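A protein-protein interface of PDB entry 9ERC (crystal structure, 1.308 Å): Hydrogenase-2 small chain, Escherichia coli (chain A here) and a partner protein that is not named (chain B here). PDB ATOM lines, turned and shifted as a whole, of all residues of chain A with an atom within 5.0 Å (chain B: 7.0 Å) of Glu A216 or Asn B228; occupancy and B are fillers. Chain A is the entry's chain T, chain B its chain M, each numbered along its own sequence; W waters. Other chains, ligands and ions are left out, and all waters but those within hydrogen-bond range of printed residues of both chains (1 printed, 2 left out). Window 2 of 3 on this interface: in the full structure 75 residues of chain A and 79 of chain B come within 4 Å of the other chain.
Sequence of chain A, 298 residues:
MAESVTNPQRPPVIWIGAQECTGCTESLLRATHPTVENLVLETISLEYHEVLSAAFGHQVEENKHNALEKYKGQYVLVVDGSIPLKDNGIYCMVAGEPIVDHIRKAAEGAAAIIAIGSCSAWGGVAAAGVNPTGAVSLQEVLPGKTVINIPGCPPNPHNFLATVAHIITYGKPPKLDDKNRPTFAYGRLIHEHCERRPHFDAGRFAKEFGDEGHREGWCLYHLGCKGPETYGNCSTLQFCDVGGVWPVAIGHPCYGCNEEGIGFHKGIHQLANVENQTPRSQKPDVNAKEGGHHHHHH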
ATOM      1  N   GLU A 212     -15.781  30.624 -15.058  1.00  0.00           N
ATOM      2  CA  GLU A 212     -16.944  31.258 -14.451  1.00  0.00           C
ATOM      3  C   GLU A 212     -18.116  30.289 -14.349  1.00  0.00           C
ATOM      4  O   GLU A 212     -18.784  30.253 -13.313  1.00  0.00           O
ATOM      5  CB  GLU A 212     -17.374  32.501 -15.235  1.00  0.00           C
ATOM      6  CG  GLU A 212     -16.589  33.730 -14.855  1.00  0.00           C
ATOM      7  CD  GLU A 212     -17.251  35.048 -15.262  1.00  0.00           C
ATOM      8  OE1 GLU A 212     -18.377  35.022 -15.856  1.00  0.00           O
ATOM      9  OE2 GLU A 212     -16.650  36.093 -14.960  1.00  0.00           O
ATOM     10  N   GLY A 213     -18.375  29.510 -15.385  1.00  0.00           N
ATOM     11  CA  GLY A 213     -19.467  28.550 -15.376  1.00  0.00           C
ATOM     12  C   GLY A 213     -19.263  27.417 -14.349  1.00  0.00           C
ATOM     13  O   GLY A 213     -20.189  26.992 -13.647  1.00  0.00           O
ATOM     14  N   HIS A 214     -18.028  26.901 -14.287  1.00  0.00           N
ATOM     15  CA  HIS A 214     -17.676  25.899 -13.292  1.00  0.00           C
ATOM     16  C   HIS A 214     -17.976  26.431 -11.884  1.00  0.00           C
ATOM     17  O   HIS A 214     -18.534  25.714 -11.044  1.00  0.00           O
ATOM     18  CB  HIS A 214     -16.188  25.592 -13.439  1.00  0.00           C
ATOM     19  CG  HIS A 214     -15.728  24.470 -12.577  1.00  0.00           C
ATOM     20  ND1 HIS A 214     -14.709  24.643 -11.682  1.00  0.00           N
ATOM     21  CD2 HIS A 214     -16.146  23.201 -12.458  1.00  0.00           C
ATOM     22  CE1 HIS A 214     -14.500  23.490 -11.059  1.00  0.00           C
ATOM     23  NE2 HIS A 214     -15.368  22.589 -11.517  1.00  0.00           N
ATOM     24  N   ARG A 215     -17.630  27.704 -11.663  1.00  0.00           N
ATOM     25  CA  ARG A 215     -17.828  28.384 -10.395  1.00  0.00           C
ATOM     26  C   ARG A 215     -19.273  28.794 -10.152  1.00  0.00           C
ATOM     27  O   ARG A 215     -19.551  29.341  -9.085  1.00  0.00           O
ATOM     28  CB  ARG A 215     -16.841  29.549 -10.273  1.00  0.00           C
ATOM     29  CG  ARG A 215     -15.427  29.035 -10.053  1.00  0.00           C
ATOM     30  CD  ARG A 215     -14.415  30.155 -10.039  1.00  0.00           C
ATOM     31  NE  ARG A 215     -14.575  30.972  -8.865  1.00  0.00           N
ATOM     32  CZ  ARG A 215     -15.020  32.223  -8.860  1.00  0.00           C
ATOM     33  NH1 ARG A 215     -15.125  32.888  -9.996  1.00  0.00           N
ATOM     34  NH2 ARG A 215     -15.295  32.811  -7.713  1.00  0.00           N
ATOM     35  N   GLU A 216     -20.157  28.487 -11.097  1.00  0.00           N
ATOM     36  CA  GLU A 216     -21.596  28.613 -10.884  1.00  0.00           C
ATOM     37  C   GLU A 216     -22.305  27.269 -10.807  1.00  0.00           C
ATOM     38  O   GLU A 216     -23.528  27.210 -10.763  1.00  0.00           O
ATOM     39  CB  GLU A 216     -22.201  29.475 -12.002  1.00  0.00           C
ATOM     40  CG  GLU A 216     -21.717  30.924 -12.013  1.00  0.00           C
ATOM     41  CD  GLU A 216     -21.953  31.761 -10.757  1.00  0.00           C
ATOM     42  OE1 GLU A 216     -22.864  31.417  -9.927  1.00  0.00           O
ATOM     43  OE2 GLU A 216     -21.181  32.737 -10.554  1.00  0.00           O
ATOM     44  N   GLY A 217     -21.556  26.152 -10.820  1.00  0.00           N
ATOM     45  CA  GLY A 217     -22.180  24.852 -10.694  1.00  0.00           C
ATOM     46  C   GLY A 217     -22.858  24.340 -11.963  1.00  0.00           C
ATOM     47  O   GLY A 217     -23.808  23.562 -11.912  1.00  0.00           O
ATOM     48  N   TRP A 218     -22.320  24.712 -13.127  1.00  0.00           N
ATOM     49  CA  TRP A 218     -22.875  24.292 -14.397  1.00  0.00           C
ATOM     50  C   TRP A 218     -22.510  22.854 -14.729  1.00  0.00           C
ATOM     51  O   TRP A 218     -21.715  22.201 -14.047  1.00  0.00           O
ATOM     52  CB  TRP A 218     -22.395  25.258 -15.493  1.00  0.00           C
ATOM     53  CG  TRP A 218     -23.023  26.615 -15.429  1.00  0.00           C
ATOM     54  CD1 TRP A 218     -23.939  27.072 -14.525  1.00  0.00           C
ATOM     55  CD2 TRP A 218     -22.799  27.699 -16.348  1.00  0.00           C
ATOM     56  NE1 TRP A 218     -24.299  28.368 -14.812  1.00  0.00           N
ATOM     57  CE2 TRP A 218     -23.608  28.777 -15.927  1.00  0.00           C
ATOM     58  CE3 TRP A 218     -22.015  27.838 -17.502  1.00  0.00           C
ATOM     59  CZ2 TRP A 218     -23.645  29.987 -16.626  1.00  0.00           C
ATOM     60  CZ3 TRP A 218     -22.058  29.034 -18.189  1.00  0.00           C
ATOM     61  CH2 TRP A 218     -22.848  30.092 -17.747  1.00  0.00           C
ATOM     62  N   ASN B 225     -12.350  21.737  -7.261  1.00  0.00           N
ATOM     63  CA  ASN B 225     -13.298  22.418  -6.378  1.00  0.00           C
ATOM     64  C   ASN B 225     -13.464  23.847  -6.886  1.00  0.00           C
ATOM     65  O   ASN B 225     -12.464  24.528  -7.109  1.00  0.00           O
ATOM     66  CB  ASN B 225     -12.785  22.501  -4.951  1.00  0.00           C
ATOM     67  CG  ASN B 225     -12.380  21.147  -4.408  1.00  0.00           C
ATOM     68  OD1 ASN B 225     -11.273  20.668  -4.658  1.00  0.00           O
ATOM     69  ND2 ASN B 225     -13.289  20.510  -3.711  1.00  0.00           N
ATOM     70  N   PRO B 226     -14.697  24.364  -7.112  1.00  0.00           N
ATOM     71  CA  PRO B 226     -14.887  25.733  -7.561  1.00  0.00           C
ATOM     72  C   PRO B 226     -15.130  26.632  -6.347  1.00  0.00           C
ATOM     73  O   PRO B 226     -16.158  26.515  -5.699  1.00  0.00           O
ATOM     74  CB  PRO B 226     -16.145  25.656  -8.442  1.00  0.00           C
ATOM     75  CG  PRO B 226     -16.699  24.251  -8.274  1.00  0.00           C
ATOM     76  CD  PRO B 226     -15.967  23.642  -7.083  1.00  0.00           C
ATOM     77  N   ILE B 227     -14.180  27.502  -6.026  1.00  0.00           N
ATOM     78  CA  ILE B 227     -14.311  28.400  -4.882  1.00  0.00           C
ATOM     79  C   ILE B 227     -15.143  29.612  -5.286  1.00  0.00           C
ATOM     80  O   ILE B 227     -14.778  30.359  -6.190  1.00  0.00           O
ATOM     81  CB  ILE B 227     -12.944  28.842  -4.355  1.00  0.00           C
ATOM     82  CG1 ILE B 227     -12.177  27.634  -3.799  1.00  0.00           C
ATOM     83  CG2 ILE B 227     -13.098  29.939  -3.310  1.00  0.00           C
ATOM     84  CD1 ILE B 227     -10.764  27.955  -3.376  1.00  0.00           C
ATOM     85  N   ASN B 228     -16.267  29.802  -4.589  1.00  0.00           N
ATOM     86  CA  ASN B 228     -17.134  30.930  -4.851  1.00  0.00           C
ATOM     87  C   ASN B 228     -18.041  31.089  -3.630  1.00  0.00           C
ATOM     88  O   ASN B 228     -19.025  30.372  -3.528  1.00  0.00           O
ATOM     89  CB  ASN B 228     -17.933  30.752  -6.129  1.00  0.00           C
ATOM     90  CG  ASN B 228     -18.782  31.965  -6.450  1.00  0.00           C
ATOM     91  OD1 ASN B 228     -18.791  32.924  -5.676  1.00  0.00           O
ATOM     92  ND2 ASN B 228     -19.479  31.909  -7.567  1.00  0.00           N
ATOM     93  N   LEU B 229     -17.700  32.023  -2.749  1.00  0.00           N
ATOM     94  CA  LEU B 229     -18.460  32.197  -1.512  1.00  0.00           C
ATOM     95  C   LEU B 229     -19.911  32.546  -1.804  1.00  0.00           C
ATOM     96  O   LEU B 229     -20.785  32.275  -0.970  1.00  0.00           O
ATOM     97  CB  LEU B 229     -17.832  33.278  -0.639  1.00  0.00           C
ATOM     98  CG  LEU B 229     -16.448  32.997  -0.062  1.00  0.00           C
ATOM     99  CD1 LEU B 229     -16.072  34.063   0.943  1.00  0.00           C
ATOM    100  CD2 LEU B 229     -16.356  31.625   0.558  1.00  0.00           C
ATOM    101  N   ASP B 230     -20.173  33.110  -2.992  1.00  0.00           N
ATOM    102  CA  ASP B 230     -21.495  33.590  -3.361  1.00  0.00           C
ATOM    103  C   ASP B 230     -22.205  32.665  -4.341  1.00  0.00           C
ATOM    104  O   ASP B 230     -23.289  32.982  -4.807  1.00  0.00           O
ATOM    105  CB  ASP B 230     -21.362  35.039  -3.840  1.00  0.00           C
ATOM    106  CG  ASP B 230     -20.880  35.918  -2.686  1.00  0.00           C
ATOM    107  OD1 ASP B 230     -21.555  35.983  -1.627  1.00  0.00           O
ATOM    108  OD2 ASP B 230     -19.776  36.458  -2.785  1.00  0.00           O
ATOM    109  N   GLY B 231     -21.628  31.477  -4.604  1.00  0.00           N
ATOM    110  CA  GLY B 231     -22.157  30.565  -5.593  1.00  0.00           C
ATOM    111  C   GLY B 231     -23.024  29.467  -4.969  1.00  0.00           C
ATOM    112  O   GLY B 231     -22.724  28.967  -3.891  1.00  0.00           O
ATOM    113  N   LEU B 232     -24.080  29.124  -5.676  1.00  0.00           N
ATOM    114  CA  LEU B 232     -24.923  27.995  -5.355  1.00  0.00           C
ATOM    115  C   LEU B 232     -24.331  26.737  -5.987  1.00  0.00           C
ATOM    116  O   LEU B 232     -23.921  26.763  -7.139  1.00  0.00           O
ATOM    117  CB  LEU B 232     -26.334  28.351  -5.848  1.00  0.00           C
ATOM    118  CG  LEU B 232     -27.450  27.367  -5.494  1.00  0.00           C
ATOM    119  CD1 LEU B 232     -28.777  28.103  -5.421  1.00  0.00           C
ATOM    120  CD2 LEU B 232     -27.537  26.262  -6.503  1.00  0.00           C
ATOM    121  N   GLY B 233     -24.257  25.631  -5.227  1.00  0.00           N
ATOM    122  CA  GLY B 233     -23.811  24.354  -5.774  1.00  0.00           C
ATOM    123  C   GLY B 233     -22.300  24.195  -5.829  1.00  0.00           C
ATOM    124  O   GLY B 233     -21.842  23.230  -6.428  1.00  0.00           O
ATOM    125  N   VAL B 234     -21.533  25.128  -5.248  1.00  0.00           N
ATOM    126  CA  VAL B 234     -20.072  25.112  -5.332  1.00  0.00           C
ATOM    127  C   VAL B 234     -19.483  25.260  -3.924  1.00  0.00           C
ATOM    128  O   VAL B 234     -20.225  25.217  -2.929  1.00  0.00           O
ATOM    129  CB  VAL B 234     -19.572  26.179  -6.328  1.00  0.00           C
ATOM    130  CG1 VAL B 234     -20.151  25.929  -7.717  1.00  0.00           C
ATOM    131  CG2 VAL B 234     -19.878  27.598  -5.847  1.00  0.00           C
ATOM    132  N   LEU B 235     -18.149  25.438  -3.829  1.00  0.00           N
ATOM    133  CA  LEU B 235     -17.486  25.524  -2.541  1.00  0.00           C
ATOM    134  C   LEU B 235     -17.629  26.951  -2.022  1.00  0.00           C
ATOM    135  O   LEU B 235     -16.849  27.858  -2.351  1.00  0.00           O
ATOM    136  CB  LEU B 235     -16.011  25.118  -2.658  1.00  0.00           C
ATOM    137  CG  LEU B 235     -15.231  25.083  -1.350  1.00  0.00           C
ATOM    138  CD1 LEU B 235     -15.903  24.148  -0.373  1.00  0.00           C
ATOM    139  CD2 LEU B 235     -13.814  24.600  -1.614  1.00  0.00           C
ATOM    140  N   ASN B 236     -18.677  27.124  -1.212  1.00  0.00           N
ATOM    141  CA  ASN B 236     -19.053  28.427  -0.700  1.00  0.00           C
ATOM    142  C   ASN B 236     -18.831  28.447   0.813  1.00  0.00           C
ATOM    143  O   ASN B 236     -18.219  27.539   1.378  1.00  0.00           O
ATOM    144  CB  ASN B 236     -20.475  28.764  -1.138  1.00  0.00           C
ATOM    145  CG  ASN B 236     -21.471  27.764  -0.589  1.00  0.00           C
ATOM    146  OD1 ASN B 236     -21.235  27.162   0.446  1.00  0.00           O
ATOM    147  ND2 ASN B 236     -22.598  27.599  -1.251  1.00  0.00           N
ATOM    148  N   LEU B 237     -19.254  29.514   1.495  1.00  0.00           N
ATOM    149  CA  LEU B 237     -18.912  29.608   2.902  1.00  0.00           C
ATOM    150  C   LEU B 237     -19.663  28.568   3.729  1.00  0.00           C
ATOM    151  O   LEU B 237     -19.131  28.067   4.712  1.00  0.00           O
ATOM    152  CB  LEU B 237     -19.169  31.026   3.419  1.00  0.00           C
ATOM    153  CG  LEU B 237     -18.648  31.268   4.834  1.00  0.00           C
ATOM    154  CD1 LEU B 237     -17.152  31.004   4.955  1.00  0.00           C
ATOM    155  CD2 LEU B 237     -18.962  32.686   5.247  1.00  0.00           C
ATOM    156  N   ILE B 450      -9.094  33.204   0.546  1.00  0.00           N
ATOM    157  CA  ILE B 450     -10.308  33.512  -0.185  1.00  0.00           C
ATOM    158  C   ILE B 450     -10.719  34.951   0.124  1.00  0.00           C
ATOM    159  O   ILE B 450     -11.201  35.649  -0.763  1.00  0.00           O
ATOM    160  CB  ILE B 450     -11.402  32.491   0.165  1.00  0.00           C
ATOM    161  CG1 ILE B 450     -11.029  31.108  -0.350  1.00  0.00           C
ATOM    162  CG2 ILE B 450     -12.740  32.957  -0.365  1.00  0.00           C
ATOM    163  CD1 ILE B 450     -11.933  29.996   0.176  1.00  0.00           C
ATOM    164  N   HIS B 455      -9.641  33.242  -5.647  1.00  0.00           N
ATOM    165  CA  HIS B 455     -10.480  32.068  -5.804  1.00  0.00           C
ATOM    166  C   HIS B 455      -9.877  31.089  -6.815  1.00  0.00           C
ATOM    167  O   HIS B 455     -10.563  30.150  -7.253  1.00  0.00           O
ATOM    168  CB  HIS B 455     -11.893  32.478  -6.224  1.00  0.00           C
ATOM    169  CG  HIS B 455     -11.933  33.246  -7.503  1.00  0.00           C
ATOM    170  ND1 HIS B 455     -11.641  32.710  -8.738  1.00  0.00           N
ATOM    171  CD2 HIS B 455     -12.252  34.543  -7.716  1.00  0.00           C
ATOM    172  CE1 HIS B 455     -11.781  33.668  -9.661  1.00  0.00           C
ATOM    173  NE2 HIS B 455     -12.187  34.766  -9.066  1.00  0.00           N
HETATM  174  O   HOH W   1     -24.293  29.557  -8.607  1.00  0.00           O
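The guanidinium group of Arg A215 sits at hydrogen-bond distance from the backbone carbonyl oxygen of Ile B227 (2.8 Å).
The side-chain amide nitrogen (ND2) of Asn B228 sits at hydrogen-bond distance from the backbone carbonyl oxygen (O) of Arg A215, at 3.0 Å.
The guanidinium group of Arg A215 is in hydrogen-bond range of a ring nitrogen (ND1) of His B455 (3.4 Å).
The backbone carbonyl oxygen (O) of Pro B226 sits at hydrogen-bond distance from the backbone NH (N) of Leu B235, at 2.9 Å.
The backbone NH of Gly B231 sits at hydrogen-bond distance from the side-chain amide oxygen of Asn B228, at 3.4 Å.
The backbone NH of Asn B228 is in hydrogen-bond range of the backbone carbonyl oxygen of Leu B235.
The backbone NH (N) of Asp B230 lies close to the side-chain amide oxygen (OD1) of Asn B228, 3.0 Å away.
Among the printed residues, pairs that only touch across the chains: His A214 with Pro B226, His A214 with Val B234, Arg A215 with Pro B226, Arg A215 with Val B234, Glu A216 with Asn B228, Glu A216 with Leu B232, Glu A216 with Val B234 and Gly A217 with Val B234.
Of the printed residues of chain B, Glu A216 touches Asn B228, Leu B232 and Val B234.
Of the printed residues of chain A, His B455 touches Arg A215 (3.4 Å).
Printed residues of chain B within 4 Å of Arg A215: Pro B226, Ile B227, Asn B228, Val B234 and His B455.
Of the printed residues of chain A, Pro B226 touches His A214 (3.5 Å) and Arg A215 (3.8 Å).
Printed residues of chain A within 4 Å of Val B234: His A214, Arg A215, Glu A216 and Gly A217.
Asn B236 touches none of the printed residues of chain A.
Gly B233 touches none of the printed residues of chain A.
The nearest printed residue of chain B that does not touch Glu A216 is Gly B231 (4.5 Å).
Printed residues of chain A that touch a printed residue of chain B: His A214, Arg A215, Glu A216 and Gly A217.
Hydrophobic or aromatic side chains of chain A within 4 Å of the printed part of chain B: His A214.
Along chain A the printed residues that touch a printed residue of chain B span positions 214 to 217.
Of the 15 printed residues of chain B, 6 touch a printed residue of chain A.
Hydrophobic or aromatic side chains of chain B within 4 Å of the printed part of chain A: Pro B226, Val B234 and His B455.
Among the printed residues, 11 pairs touch across the chains.
Among the printed residues, no Asp or Glu carboxylate lies within 4 Å of a Lys or Arg side-chain nitrogen of the other chain.
Water W1 lies within hydrogen-bond range of the side-chain carboxylate (OE1) of Glu A216 (2.7 Å) and the backbone NH (N) of Leu B232 (3.0 Å).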
